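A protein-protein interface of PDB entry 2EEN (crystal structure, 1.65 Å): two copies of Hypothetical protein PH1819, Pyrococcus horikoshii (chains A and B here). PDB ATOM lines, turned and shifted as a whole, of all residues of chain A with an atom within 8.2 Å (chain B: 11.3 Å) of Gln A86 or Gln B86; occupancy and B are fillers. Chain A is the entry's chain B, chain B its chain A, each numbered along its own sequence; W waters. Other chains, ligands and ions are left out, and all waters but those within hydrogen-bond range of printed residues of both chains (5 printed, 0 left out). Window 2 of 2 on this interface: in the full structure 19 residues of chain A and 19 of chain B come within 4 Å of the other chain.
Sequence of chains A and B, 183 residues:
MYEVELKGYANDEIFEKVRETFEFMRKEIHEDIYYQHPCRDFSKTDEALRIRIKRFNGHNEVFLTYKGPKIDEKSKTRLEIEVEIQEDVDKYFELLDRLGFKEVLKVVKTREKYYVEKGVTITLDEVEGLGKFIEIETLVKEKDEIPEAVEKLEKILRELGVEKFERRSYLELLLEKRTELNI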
ATOM      1  N   ASN A  60       9.038   8.381  23.603  1.00  0.00           N
ATOM      2  CA  ASN A  60       8.995   9.444  22.610  1.00  0.00           C
ATOM      3  C   ASN A  60      10.341   9.599  21.924  1.00  0.00           C
ATOM      4  O   ASN A  60      11.390   9.410  22.539  1.00  0.00           O
ATOM      5  CB  ASN A  60       8.647  10.794  23.262  1.00  0.00           C
ATOM      6  CG  ASN A  60       7.207  10.881  23.726  1.00  0.00           C
ATOM      7  OD1 ASN A  60       6.411   9.970  23.477  1.00  0.00           O
ATOM      8  ND2 ASN A  60       6.863  11.964  24.404  1.00  0.00           N
ATOM      9  N   GLU A  61      10.299   9.932  20.639  1.00  0.00           N
ATOM     10  CA  GLU A  61      11.506  10.188  19.870  1.00  0.00           C
ATOM     11  C   GLU A  61      11.234  11.530  19.209  1.00  0.00           C
ATOM     12  O   GLU A  61      10.097  11.829  18.851  1.00  0.00           O
ATOM     13  CB  GLU A  61      11.746   9.104  18.816  1.00  0.00           C
ATOM     14  CG  GLU A  61      11.797   7.702  19.398  1.00  0.00           C
ATOM     15  CD  GLU A  61      12.710   6.777  18.621  1.00  0.00           C
ATOM     16  OE1 GLU A  61      12.860   6.973  17.397  1.00  0.00           O
ATOM     17  OE2 GLU A  61      13.268   5.842  19.238  1.00  0.00           O
ATOM     18  N   VAL A  62      12.268  12.347  19.066  1.00  0.00           N
ATOM     19  CA  VAL A  62      12.089  13.668  18.481  1.00  0.00           C
ATOM     20  C   VAL A  62      13.026  13.875  17.307  1.00  0.00           C
ATOM     21  O   VAL A  62      14.197  13.508  17.376  1.00  0.00           O
ATOM     22  CB  VAL A  62      12.338  14.767  19.537  1.00  0.00           C
ATOM     23  CG1 VAL A  62      12.078  16.148  18.933  1.00  0.00           C
ATOM     24  CG2 VAL A  62      11.434  14.538  20.744  1.00  0.00           C
ATOM     25  N   PHE A  63      12.505  14.462  16.231  1.00  0.00           N
ATOM     26  CA  PHE A  63      13.309  14.716  15.043  1.00  0.00           C
ATOM     27  C   PHE A  63      13.125  16.118  14.501  1.00  0.00           C
ATOM     28  O   PHE A  63      12.052  16.705  14.606  1.00  0.00           O
ATOM     29  CB  PHE A  63      12.945  13.729  13.942  1.00  0.00           C
ATOM     30  CG  PHE A  63      13.196  12.307  14.310  1.00  0.00           C
ATOM     31  CD1 PHE A  63      12.245  11.589  15.022  1.00  0.00           C
ATOM     32  CD2 PHE A  63      14.400  11.693  13.987  1.00  0.00           C
ATOM     33  CE1 PHE A  63      12.492  10.280  15.414  1.00  0.00           C
ATOM     34  CE2 PHE A  63      14.655  10.380  14.375  1.00  0.00           C
ATOM     35  CZ  PHE A  63      13.696   9.674  15.090  1.00  0.00           C
ATOM     36  N   VAL A  83      17.616  14.982  11.560  1.00  0.00           N
ATOM     37  CA  VAL A  83      18.473  14.661  12.692  1.00  0.00           C
ATOM     38  C   VAL A  83      17.598  14.370  13.898  1.00  0.00           C
ATOM     39  O   VAL A  83      16.522  14.953  14.055  1.00  0.00           O
ATOM     40  CB  VAL A  83      19.444  15.814  13.035  1.00  0.00           C
ATOM     41  CG1 VAL A  83      20.411  16.024  11.885  1.00  0.00           C
ATOM     42  CG2 VAL A  83      18.674  17.094  13.331  1.00  0.00           C
ATOM     43  N   GLU A  84      18.051  13.456  14.744  1.00  0.00           N
ATOM     44  CA  GLU A  84      17.284  13.120  15.929  1.00  0.00           C
ATOM     45  C   GLU A  84      17.724  13.971  17.108  1.00  0.00           C
ATOM     46  O   GLU A  84      18.915  14.174  17.337  1.00  0.00           O
ATOM     47  CB  GLU A  84      17.438  11.633  16.284  1.00  0.00           C
ATOM     48  CG  GLU A  84      16.598  11.229  17.503  1.00  0.00           C
ATOM     49  CD  GLU A  84      16.738   9.764  17.888  1.00  0.00           C
ATOM     50  OE1 GLU A  84      17.665   9.097  17.386  1.00  0.00           O
ATOM     51  OE2 GLU A  84      15.930   9.286  18.714  1.00  0.00           O
ATOM     52  N   ILE A  85      16.744  14.480  17.845  1.00  0.00           N
ATOM     53  CA  ILE A  85      17.000  15.295  19.024  1.00  0.00           C
ATOM     54  C   ILE A  85      16.888  14.315  20.186  1.00  0.00           C
ATOM     55  O   ILE A  85      15.796  13.896  20.545  1.00  0.00           O
ATOM     56  CB  ILE A  85      15.943  16.413  19.150  1.00  0.00           C
ATOM     57  CG1 ILE A  85      16.117  17.406  17.994  1.00  0.00           C
ATOM     58  CG2 ILE A  85      16.064  17.111  20.504  1.00  0.00           C
ATOM     59  CD1 ILE A  85      15.054  18.480  17.926  1.00  0.00           C
ATOM     60  N   GLN A  86      18.029  13.936  20.753  1.00  0.00           N
ATOM     61  CA  GLN A  86      18.058  12.975  21.848  1.00  0.00           C
ATOM     62  C   GLN A  86      17.871  13.625  23.211  1.00  0.00           C
ATOM     63  O   GLN A  86      17.525  12.960  24.184  1.00  0.00           O
ATOM     64  CB  GLN A  86      19.380  12.203  21.819  1.00  0.00           C
ATOM     65  CG  GLN A  86      19.688  11.559  20.474  1.00  0.00           C
ATOM     66  CD  GLN A  86      21.020  10.832  20.460  1.00  0.00           C
ATOM     67  OE1 GLN A  86      21.479  10.373  19.412  1.00  0.00           O
ATOM     68  NE2 GLN A  86      21.648  10.721  21.628  1.00  0.00           N
ATOM     69  N   GLU A  87      18.099  14.930  23.278  1.00  0.00           N
ATOM     70  CA  GLU A  87      17.949  15.656  24.528  1.00  0.00           C
ATOM     71  C   GLU A  87      17.713  17.136  24.269  1.00  0.00           C
ATOM     72  O   GLU A  87      17.953  17.631  23.166  1.00  0.00           O
ATOM     73  CB  GLU A  87      19.203  15.473  25.390  1.00  0.00           C
ATOM     74  CG  GLU A  87      20.509  15.653  24.631  1.00  0.00           C
ATOM     75  CD  GLU A  87      21.730  15.501  25.522  1.00  0.00           C
ATOM     76  OE1 GLU A  87      21.815  14.487  26.248  1.00  0.00           O
ATOM     77  OE2 GLU A  87      22.608  16.391  25.488  1.00  0.00           O
ATOM     78  N   ASP A  88      17.222  17.829  25.291  1.00  0.00           N
ATOM     79  CA  ASP A  88      16.971  19.264  25.220  1.00  0.00           C
ATOM     80  C   ASP A  88      16.066  19.752  24.087  1.00  0.00           C
ATOM     81  O   ASP A  88      16.355  20.779  23.477  1.00  0.00           O
ATOM     82  CB  ASP A  88      18.303  20.023  25.125  1.00  0.00           C
ATOM     83  CG  ASP A  88      19.182  19.823  26.343  1.00  0.00           C
ATOM     84  OD1 ASP A  88      18.673  19.965  27.476  1.00  0.00           O
ATOM     85  OD2 ASP A  88      20.388  19.536  26.166  1.00  0.00           O
ATOM     86  N   VAL A  89      14.972  19.054  23.802  1.00  0.00           N
ATOM     87  CA  VAL A  89      14.099  19.518  22.731  1.00  0.00           C
ATOM     88  C   VAL A  89      13.603  20.941  23.022  1.00  0.00           C
ATOM     89  O   VAL A  89      13.366  21.726  22.102  1.00  0.00           O
ATOM     90  CB  VAL A  89      12.879  18.585  22.531  1.00  0.00           C
ATOM     91  CG1 VAL A  89      11.993  18.608  23.760  1.00  0.00           C
ATOM     92  CG2 VAL A  89      12.108  19.008  21.290  1.00  0.00           C
ATOM     93  N   TYR A  92      15.815  23.307  21.499  1.00  0.00           N
ATOM     94  CA  TYR A  92      15.667  23.439  20.056  1.00  0.00           C
ATOM     95  C   TYR A  92      14.496  24.369  19.760  1.00  0.00           C
ATOM     96  O   TYR A  92      14.554  25.168  18.822  1.00  0.00           O
ATOM     97  CB  TYR A  92      15.443  22.076  19.385  1.00  0.00           C
ATOM     98  CG  TYR A  92      16.712  21.268  19.199  1.00  0.00           C
ATOM     99  CD1 TYR A  92      17.308  20.605  20.274  1.00  0.00           C
ATOM    100  CD2 TYR A  92      17.334  21.189  17.953  1.00  0.00           C
ATOM    101  CE1 TYR A  92      18.493  19.883  20.112  1.00  0.00           C
ATOM    102  CE2 TYR A  92      18.521  20.468  17.780  1.00  0.00           C
ATOM    103  CZ  TYR A  92      19.092  19.820  18.864  1.00  0.00           C
ATOM    104  OH  TYR A  92      20.261  19.099  18.714  1.00  0.00           O
ATOM    105  N   ILE B  51      28.887  26.492  15.425  1.00  0.00           N
ATOM    106  CA  ILE B  51      28.998  25.060  15.621  1.00  0.00           C
ATOM    107  C   ILE B  51      30.432  24.902  16.078  1.00  0.00           C
ATOM    108  O   ILE B  51      31.365  25.344  15.399  1.00  0.00           O
ATOM    109  CB  ILE B  51      28.778  24.243  14.347  1.00  0.00           C
ATOM    110  CG1 ILE B  51      27.279  24.155  14.065  1.00  0.00           C
ATOM    111  CG2 ILE B  51      29.350  22.839  14.536  1.00  0.00           C
ATOM    112  CD1 ILE B  51      26.927  23.468  12.775  1.00  0.00           C
ATOM    113  N   ARG B  52      30.598  24.300  17.249  1.00  0.00           N
ATOM    114  CA  ARG B  52      31.916  24.080  17.816  1.00  0.00           C
ATOM    115  C   ARG B  52      32.274  22.616  17.876  1.00  0.00           C
ATOM    116  O   ARG B  52      31.472  21.789  18.306  1.00  0.00           O
ATOM    117  CB  ARG B  52      31.993  24.635  19.236  1.00  0.00           C
ATOM    118  CG  ARG B  52      33.141  24.042  20.045  1.00  0.00           C
ATOM    119  CD  ARG B  52      33.296  24.776  21.357  1.00  0.00           C
ATOM    120  NE  ARG B  52      33.635  26.174  21.117  1.00  0.00           N
ATOM    121  CZ  ARG B  52      33.680  27.109  22.058  1.00  0.00           C
ATOM    122  NH1 ARG B  52      33.402  26.807  23.322  1.00  0.00           N
ATOM    123  NH2 ARG B  52      34.013  28.349  21.731  1.00  0.00           N
ATOM    124  N   ILE B  53      33.484  22.304  17.431  1.00  0.00           N
ATOM    125  CA  ILE B  53      33.990  20.944  17.507  1.00  0.00           C
ATOM    126  C   ILE B  53      35.061  21.034  18.582  1.00  0.00           C
ATOM    127  O   ILE B  53      36.013  21.805  18.460  1.00  0.00           O
ATOM    128  CB  ILE B  53      34.612  20.477  16.179  1.00  0.00           C
ATOM    129  CG1 ILE B  53      33.542  20.463  15.082  1.00  0.00           C
ATOM    130  CG2 ILE B  53      35.205  19.080  16.354  1.00  0.00           C
ATOM    131  CD1 ILE B  53      34.067  20.082  13.706  1.00  0.00           C
ATOM    132  N   LYS B  54      34.877  20.262  19.646  1.00  0.00           N
ATOM    133  CA  LYS B  54      35.791  20.253  20.777  1.00  0.00           C
ATOM    134  C   LYS B  54      36.517  18.913  20.816  1.00  0.00           C
ATOM    135  O   LYS B  54      35.884  17.858  20.823  1.00  0.00           O
ATOM    136  CB  LYS B  54      34.979  20.465  22.059  1.00  0.00           C
ATOM    137  CG  LYS B  54      35.779  20.641  23.335  1.00  0.00           C
ATOM    138  CD  LYS B  54      34.836  20.793  24.526  1.00  0.00           C
ATOM    139  CE  LYS B  54      33.943  22.020  24.384  1.00  0.00           C
ATOM    140  NZ  LYS B  54      32.928  22.112  25.478  1.00  0.00           N
ATOM    141  N   HIS B  59      38.726  12.283  22.436  1.00  0.00           N
ATOM    142  CA  HIS B  59      37.294  12.489  22.269  1.00  0.00           C
ATOM    143  C   HIS B  59      36.994  13.696  21.387  1.00  0.00           C
ATOM    144  O   HIS B  59      37.825  14.585  21.224  1.00  0.00           O
ATOM    145  CB  HIS B  59      36.630  12.716  23.629  1.00  0.00           C
ATOM    146  CG  HIS B  59      36.911  11.646  24.633  1.00  0.00           C
ATOM    147  ND1 HIS B  59      36.548  10.329  24.442  1.00  0.00           N
ATOM    148  CD2 HIS B  59      37.505  11.697  25.850  1.00  0.00           C
ATOM    149  CE1 HIS B  59      36.905   9.619  25.497  1.00  0.00           C
ATOM    150  NE2 HIS B  59      37.487  10.425  26.366  1.00  0.00           N
ATOM    151  N   ASN B  60      35.789  13.713  20.830  1.00  0.00           N
ATOM    152  CA  ASN B  60      35.326  14.807  19.990  1.00  0.00           C
ATOM    153  C   ASN B  60      33.889  15.113  20.399  1.00  0.00           C
ATOM    154  O   ASN B  60      33.043  14.221  20.404  1.00  0.00           O
ATOM    155  CB  ASN B  60      35.341  14.415  18.508  1.00  0.00           C
ATOM    156  CG  ASN B  60      36.742  14.235  17.961  1.00  0.00           C
ATOM    157  OD1 ASN B  60      37.517  15.189  17.871  1.00  0.00           O
ATOM    158  ND2 ASN B  60      37.076  13.005  17.589  1.00  0.00           N
ATOM    159  N   GLU B  61      33.623  16.362  20.764  1.00  0.00           N
ATOM    160  CA  GLU B  61      32.272  16.776  21.132  1.00  0.00           C
ATOM    161  C   GLU B  61      31.918  17.920  20.201  1.00  0.00           C
ATOM    162  O   GLU B  61      32.783  18.704  19.820  1.00  0.00           O
ATOM    163  CB  GLU B  61      32.199  17.264  22.578  1.00  0.00           C
ATOM    164  CG  GLU B  61      32.479  16.203  23.631  1.00  0.00           C
ATOM    165  CD  GLU B  61      32.174  16.701  25.035  1.00  0.00           C
ATOM    166  OE1 GLU B  61      32.540  17.851  25.356  1.00  0.00           O
ATOM    167  OE2 GLU B  61      31.574  15.938  25.821  1.00  0.00           O
ATOM    168  N   VAL B  62      30.649  18.012  19.828  1.00  0.00           N
ATOM    169  CA  VAL B  62      30.215  19.058  18.921  1.00  0.00           C
ATOM    170  C   VAL B  62      29.009  19.753  19.513  1.00  0.00           C
ATOM    171  O   VAL B  62      28.114  19.105  20.034  1.00  0.00           O
ATOM    172  CB  VAL B  62      29.835  18.474  17.557  1.00  0.00           C
ATOM    173  CG1 VAL B  62      29.443  19.589  16.606  1.00  0.00           C
ATOM    174  CG2 VAL B  62      31.009  17.673  16.999  1.00  0.00           C
ATOM    175  N   PHE B  63      28.992  21.078  19.434  1.00  0.00           N
ATOM    176  CA  PHE B  63      27.882  21.834  19.992  1.00  0.00           C
ATOM    177  C   PHE B  63      27.395  22.906  19.036  1.00  0.00           C
ATOM    178  O   PHE B  63      28.174  23.466  18.267  1.00  0.00           O
ATOM    179  CB  PHE B  63      28.296  22.517  21.304  1.00  0.00           C
ATOM    180  CG  PHE B  63      28.820  21.571  22.348  1.00  0.00           C
ATOM    181  CD1 PHE B  63      30.148  21.156  22.327  1.00  0.00           C
ATOM    182  CD2 PHE B  63      27.979  21.079  23.335  1.00  0.00           C
ATOM    183  CE1 PHE B  63      30.632  20.258  23.284  1.00  0.00           C
ATOM    184  CE2 PHE B  63      28.449  20.182  24.295  1.00  0.00           C
ATOM    185  CZ  PHE B  63      29.782  19.771  24.268  1.00  0.00           C
ATOM    186  N   LEU B  64      26.094  23.166  19.081  1.00  0.00           N
ATOM    187  CA  LEU B  64      25.472  24.216  18.286  1.00  0.00           C
ATOM    188  C   LEU B  64      25.065  25.226  19.350  1.00  0.00           C
ATOM    189  O   LEU B  64      24.315  24.901  20.273  1.00  0.00           O
ATOM    190  CB  LEU B  64      24.235  23.693  17.553  1.00  0.00           C
ATOM    191  CG  LEU B  64      23.368  24.756  16.873  1.00  0.00           C
ATOM    192  CD1 LEU B  64      24.178  25.518  15.831  1.00  0.00           C
ATOM    193  CD2 LEU B  64      22.183  24.082  16.205  1.00  0.00           C
ATOM    194  N   GLU B  82      22.480  26.310  24.074  1.00  0.00           N
ATOM    195  CA  GLU B  82      23.429  25.370  23.516  1.00  0.00           C
ATOM    196  C   GLU B  82      22.920  23.952  23.575  1.00  0.00           C
ATOM    197  O   GLU B  82      22.362  23.519  24.584  1.00  0.00           O
ATOM    198  CB  GLU B  82      24.751  25.467  24.272  1.00  0.00           C
ATOM    199  CG  GLU B  82      25.805  24.460  23.857  1.00  0.00           C
ATOM    200  CD  GLU B  82      27.179  24.838  24.373  1.00  0.00           C
ATOM    201  OE1 GLU B  82      27.713  25.878  23.929  1.00  0.00           O
ATOM    202  OE2 GLU B  82      27.725  24.109  25.226  1.00  0.00           O
ATOM    203  N   VAL B  83      23.104  23.238  22.476  1.00  0.00           N
ATOM    204  CA  VAL B  83      22.702  21.847  22.407  1.00  0.00           C
ATOM    205  C   VAL B  83      23.898  21.077  21.893  1.00  0.00           C
ATOM    206  O   VAL B  83      24.716  21.606  21.133  1.00  0.00           O
ATOM    207  CB  VAL B  83      21.516  21.636  21.453  1.00  0.00           C
ATOM    208  CG1 VAL B  83      20.294  22.360  22.001  1.00  0.00           C
ATOM    209  CG2 VAL B  83      21.858  22.138  20.059  1.00  0.00           C
ATOM    210  N   GLU B  84      24.007  19.829  22.321  1.00  0.00           N
ATOM    211  CA  GLU B  84      25.112  19.008  21.887  1.00  0.00           C
ATOM    212  C   GLU B  84      24.697  18.176  20.690  1.00  0.00           C
ATOM    213  O   GLU B  84      23.624  17.561  20.689  1.00  0.00           O
ATOM    214  CB  GLU B  84      25.577  18.087  23.017  1.00  0.00           C
ATOM    215  CG  GLU B  84      26.944  17.478  22.745  1.00  0.00           C
ATOM    216  CD  GLU B  84      27.441  16.595  23.870  1.00  0.00           C
ATOM    217  OE1 GLU B  84      27.043  16.827  25.032  1.00  0.00           O
ATOM    218  OE2 GLU B  84      28.246  15.681  23.590  1.00  0.00           O
ATOM    219  N   ILE B  85      25.541  18.184  19.664  1.00  0.00           N
ATOM    220  CA  ILE B  85      25.308  17.405  18.458  1.00  0.00           C
ATOM    221  C   ILE B  85      26.007  16.077  18.732  1.00  0.00           C
ATOM    222  O   ILE B  85      27.228  15.986  18.671  1.00  0.00           O
ATOM    223  CB  ILE B  85      25.926  18.095  17.223  1.00  0.00           C
ATOM    224  CG1 ILE B  85      25.134  19.364  16.895  1.00  0.00           C
ATOM    225  CG2 ILE B  85      25.935  17.135  16.034  1.00  0.00           C
ATOM    226  CD1 ILE B  85      25.821  20.290  15.916  1.00  0.00           C
ATOM    227  N   GLN B  86      25.219  15.056  19.052  1.00  0.00           N
ATOM    228  CA  GLN B  86      25.766  13.745  19.385  1.00  0.00           C
ATOM    229  C   GLN B  86      26.059  12.854  18.188  1.00  0.00           C
ATOM    230  O   GLN B  86      26.813  11.882  18.293  1.00  0.00           O
ATOM    231  CB  GLN B  86      24.816  13.029  20.347  1.00  0.00           C
ATOM    232  CG  GLN B  86      24.612  13.773  21.659  1.00  0.00           C
ATOM    233  CD  GLN B  86      23.665  13.056  22.597  1.00  0.00           C
ATOM    234  OE1 GLN B  86      23.908  11.914  22.991  1.00  0.00           O
ATOM    235  NE2 GLN B  86      22.576  13.722  22.961  1.00  0.00           N
ATOM    236  N   GLU B  87      25.464  13.187  17.049  1.00  0.00           N
ATOM    237  CA  GLU B  87      25.657  12.421  15.824  1.00  0.00           C
ATOM    238  C   GLU B  87      25.253  13.252  14.617  1.00  0.00           C
ATOM    239  O   GLU B  87      24.646  14.315  14.758  1.00  0.00           O
ATOM    240  CB  GLU B  87      24.821  11.138  15.864  1.00  0.00           C
ATOM    241  CG  GLU B  87      23.366  11.364  16.237  1.00  0.00           C
ATOM    242  CD  GLU B  87      22.524  10.105  16.133  1.00  0.00           C
ATOM    243  OE1 GLU B  87      22.947   9.055  16.665  1.00  0.00           O
ATOM    244  OE2 GLU B  87      21.434  10.168  15.526  1.00  0.00           O
ATOM    245  N   ASP B  88      25.603  12.759  13.433  1.00  0.00           N
ATOM    246  CA  ASP B  88      25.276  13.427  12.177  1.00  0.00           C
ATOM    247  C   ASP B  88      25.696  14.890  12.133  1.00  0.00           C
ATOM    248  O   ASP B  88      24.910  15.752  11.737  1.00  0.00           O
ATOM    249  CB  ASP B  88      23.774  13.334  11.906  1.00  0.00           C
ATOM    250  CG  ASP B  88      23.283  11.905  11.838  1.00  0.00           C
ATOM    251  OD1 ASP B  88      23.912  11.094  11.128  1.00  0.00           O
ATOM    252  OD2 ASP B  88      22.260  11.599  12.486  1.00  0.00           O
ATOM    253  N   VAL B  89      26.933  15.170  12.525  1.00  0.00           N
ATOM    254  CA  VAL B  89      27.432  16.537  12.518  1.00  0.00           C
ATOM    255  C   VAL B  89      27.266  17.159  11.135  1.00  0.00           C
ATOM    256  O   VAL B  89      26.870  18.319  11.001  1.00  0.00           O
ATOM    257  CB  VAL B  89      28.924  16.590  12.895  1.00  0.00           C
ATOM    258  CG1 VAL B  89      29.387  18.033  12.959  1.00  0.00           C
ATOM    259  CG2 VAL B  89      29.150  15.892  14.226  1.00  0.00           C
ATOM    260  N   ASP B  90      27.569  16.380  10.102  1.00  0.00           N
ATOM    261  CA  ASP B  90      27.454  16.878   8.741  1.00  0.00           C
ATOM    262  C   ASP B  90      26.041  17.314   8.391  1.00  0.00           C
ATOM    263  O   ASP B  90      25.851  18.231   7.598  1.00  0.00           O
ATOM    264  CB  ASP B  90      27.941  15.823   7.747  1.00  0.00           C
ATOM    265  CG  ASP B  90      29.434  15.587   7.847  1.00  0.00           C
ATOM    266  OD1 ASP B  90      30.150  16.525   8.254  1.00  0.00           O
ATOM    267  OD2 ASP B  90      29.894  14.475   7.509  1.00  0.00           O
ATOM    268  N   LYS B  91      25.046  16.661   8.981  1.00  0.00           N
ATOM    269  CA  LYS B  91      23.668  17.033   8.704  1.00  0.00           C
ATOM    270  C   LYS B  91      23.358  18.411   9.267  1.00  0.00           C
ATOM    271  O   LYS B  91      22.608  19.180   8.657  1.00  0.00           O
ATOM    272  CB  LYS B  91      22.707  16.000   9.286  1.00  0.00           C
ATOM    273  CG  LYS B  91      22.825  14.654   8.606  1.00  0.00           C
ATOM    274  CD  LYS B  91      21.705  13.733   9.025  1.00  0.00           C
ATOM    275  CE  LYS B  91      21.707  12.467   8.191  1.00  0.00           C
ATOM    276  NZ  LYS B  91      20.528  11.611   8.514  1.00  0.00           N
ATOM    277  N   TYR B  92      23.928  18.729  10.426  1.00  0.00           N
ATOM    278  CA  TYR B  92      23.694  20.044  11.007  1.00  0.00           C
ATOM    279  C   TYR B  92      24.322  21.103  10.103  1.00  0.00           C
ATOM    280  O   TYR B  92      23.737  22.159   9.871  1.00  0.00           O
ATOM    281  CB  TYR B  92      24.269  20.123  12.427  1.00  0.00           C
ATOM    282  CG  TYR B  92      23.396  19.455  13.471  1.00  0.00           C
ATOM    283  CD1 TYR B  92      23.470  18.082  13.705  1.00  0.00           C
ATOM    284  CD2 TYR B  92      22.476  20.198  14.211  1.00  0.00           C
ATOM    285  CE1 TYR B  92      22.650  17.466  14.654  1.00  0.00           C
ATOM    286  CE2 TYR B  92      21.655  19.593  15.158  1.00  0.00           C
ATOM    287  CZ  TYR B  92      21.747  18.228  15.375  1.00  0.00           C
ATOM    288  OH  TYR B  92      20.940  17.630  16.323  1.00  0.00           O
ATOM    289  N   PHE B  93      25.511  20.817   9.580  1.00  0.00           N
ATOM    290  CA  PHE B  93      26.162  21.756   8.674  1.00  0.00           C
ATOM    291  C   PHE B  93      25.291  21.958   7.439  1.00  0.00           C
ATOM    292  O   PHE B  93      25.114  23.077   6.959  1.00  0.00           O
ATOM    293  CB  PHE B  93      27.533  21.234   8.240  1.00  0.00           C
ATOM    294  CG  PHE B  93      28.599  21.395   9.278  1.00  0.00           C
ATOM    295  CD1 PHE B  93      28.922  22.653   9.768  1.00  0.00           C
ATOM    296  CD2 PHE B  93      29.283  20.290   9.769  1.00  0.00           C
ATOM    297  CE1 PHE B  93      29.910  22.810  10.733  1.00  0.00           C
ATOM    298  CE2 PHE B  93      30.273  20.439  10.735  1.00  0.00           C
ATOM    299  CZ  PHE B  93      30.584  21.703  11.217  1.00  0.00           C
HETATM  300  O   HOH W   1      21.867  18.786  24.037  1.00  0.00           O
HETATM  301  O   HOH W   2      22.538  21.515  26.528  1.00  0.00           O
HETATM  302  O   HOH W   3      21.131  17.992  20.944  1.00  0.00           O
HETATM  303  O   HOH W   4      21.195  15.092  16.285  1.00  0.00           O
HETATM  304  O   HOH W   5      20.695  12.408  14.315  1.00  0.00           O
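Hydrophobic or aromatic side chains of chain B within 4 Å of the printed part of chain A: Val B83 and Tyr B92. Among the printed residues, 7 pairs touch across the chains.
Among the printed residues, pairs that only touch across the chains: Val A83 with Lys B91 (3.5 Å), Val A83 with Tyr B92 (3.8 Å) and Tyr A92 with Val B83 (3.6 Å).
The side-chain hydroxyl (OH) of Tyr B92 lies within hydrogen-bond range of the side-chain hydroxyl (OH) of Tyr A92 (2.9 Å). NE2 of Gln A86 lies within hydrogen-bond range of OE1 of Gln B86. OE1 of Glu B87 sits close to OE1 of Gln A86. NE2 of Gln B86 lies close to OE1 of Glu A87 (3.5 Å).
No residue of chain B comes within 4 Å of Val A62. Of the printed residues of chain B, Val A83 touches Lys B91 (3.5 Å) and Tyr B92 (3.8 Å). Ile A85 touches none of the printed residues of chain B. Of chain B, only Gln B86 and Glu B87 come within 4 Å of Gln A86. Glu A87 touches just one residue of chain B: Gln B86 (3.2 Å). Of chain A, only Gln A86 and Glu A87 come within 4 Å of Gln B86. Of the printed residues of chain A, Glu B87 touches Gln A86 (3.4 Å). Printed residues of chain A within 4 Å of Lys B91: Val A83 (3.5 Å). Of the printed residues of chain A, Tyr B92 touches Val A83 (3.8 Å) and Tyr A92 (2.9 Å). The nearest residue of chain B that does not touch Gln A86 is Tyr B92 (6.5 Å). The nearest residue of chain A that does not touch Gln B86 is Ile A85 (6.4 Å).
Val A83 touches Tyr B92, and with the chains exchanged Tyr A92 touches Val B83. Gln A86 touches its own counterpart, Gln B86. Gln A86 touches Glu B87, and with the chains exchanged Glu A87 touches Gln B86. Tyr A92 touches its own counterpart, Tyr B92. 12 positions are printed for both chains. Of the 7 pairs that touch across the chains among the printed residues, 6 have their exchanged pair printed and touching as well.
Water W5 lies within hydrogen-bond range of the side-chain carboxylate of Asp B88, the side-chain carboxylate of Glu B87 and the backbone NH of Glu A84. Water W3 bridges O of Glu B84 (2.5 Å) and OH of Tyr A92 (2.6 Å). Water W4 lies within hydrogen-bond range of the side-chain hydroxyl of Tyr B92 (2.6 Å) and the backbone carbonyl oxygen of Glu A84 (2.7 Å). Water W1 lies within hydrogen-bond range of OD2 of Asp A88 (2.7 Å), OE2 of Glu A87 (2.9 Å) and N of Glu B84 (2.9 Å). Water W2 lies within hydrogen-bond range of the backbone carbonyl oxygen of Glu B82 and the side-chain carboxylate of Asp A88.
The backbone carbonyl oxygen (O) of Val B83 is in hydrogen-bond range of the backbone NH (N) of Leu B64, 2.9 Å away.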
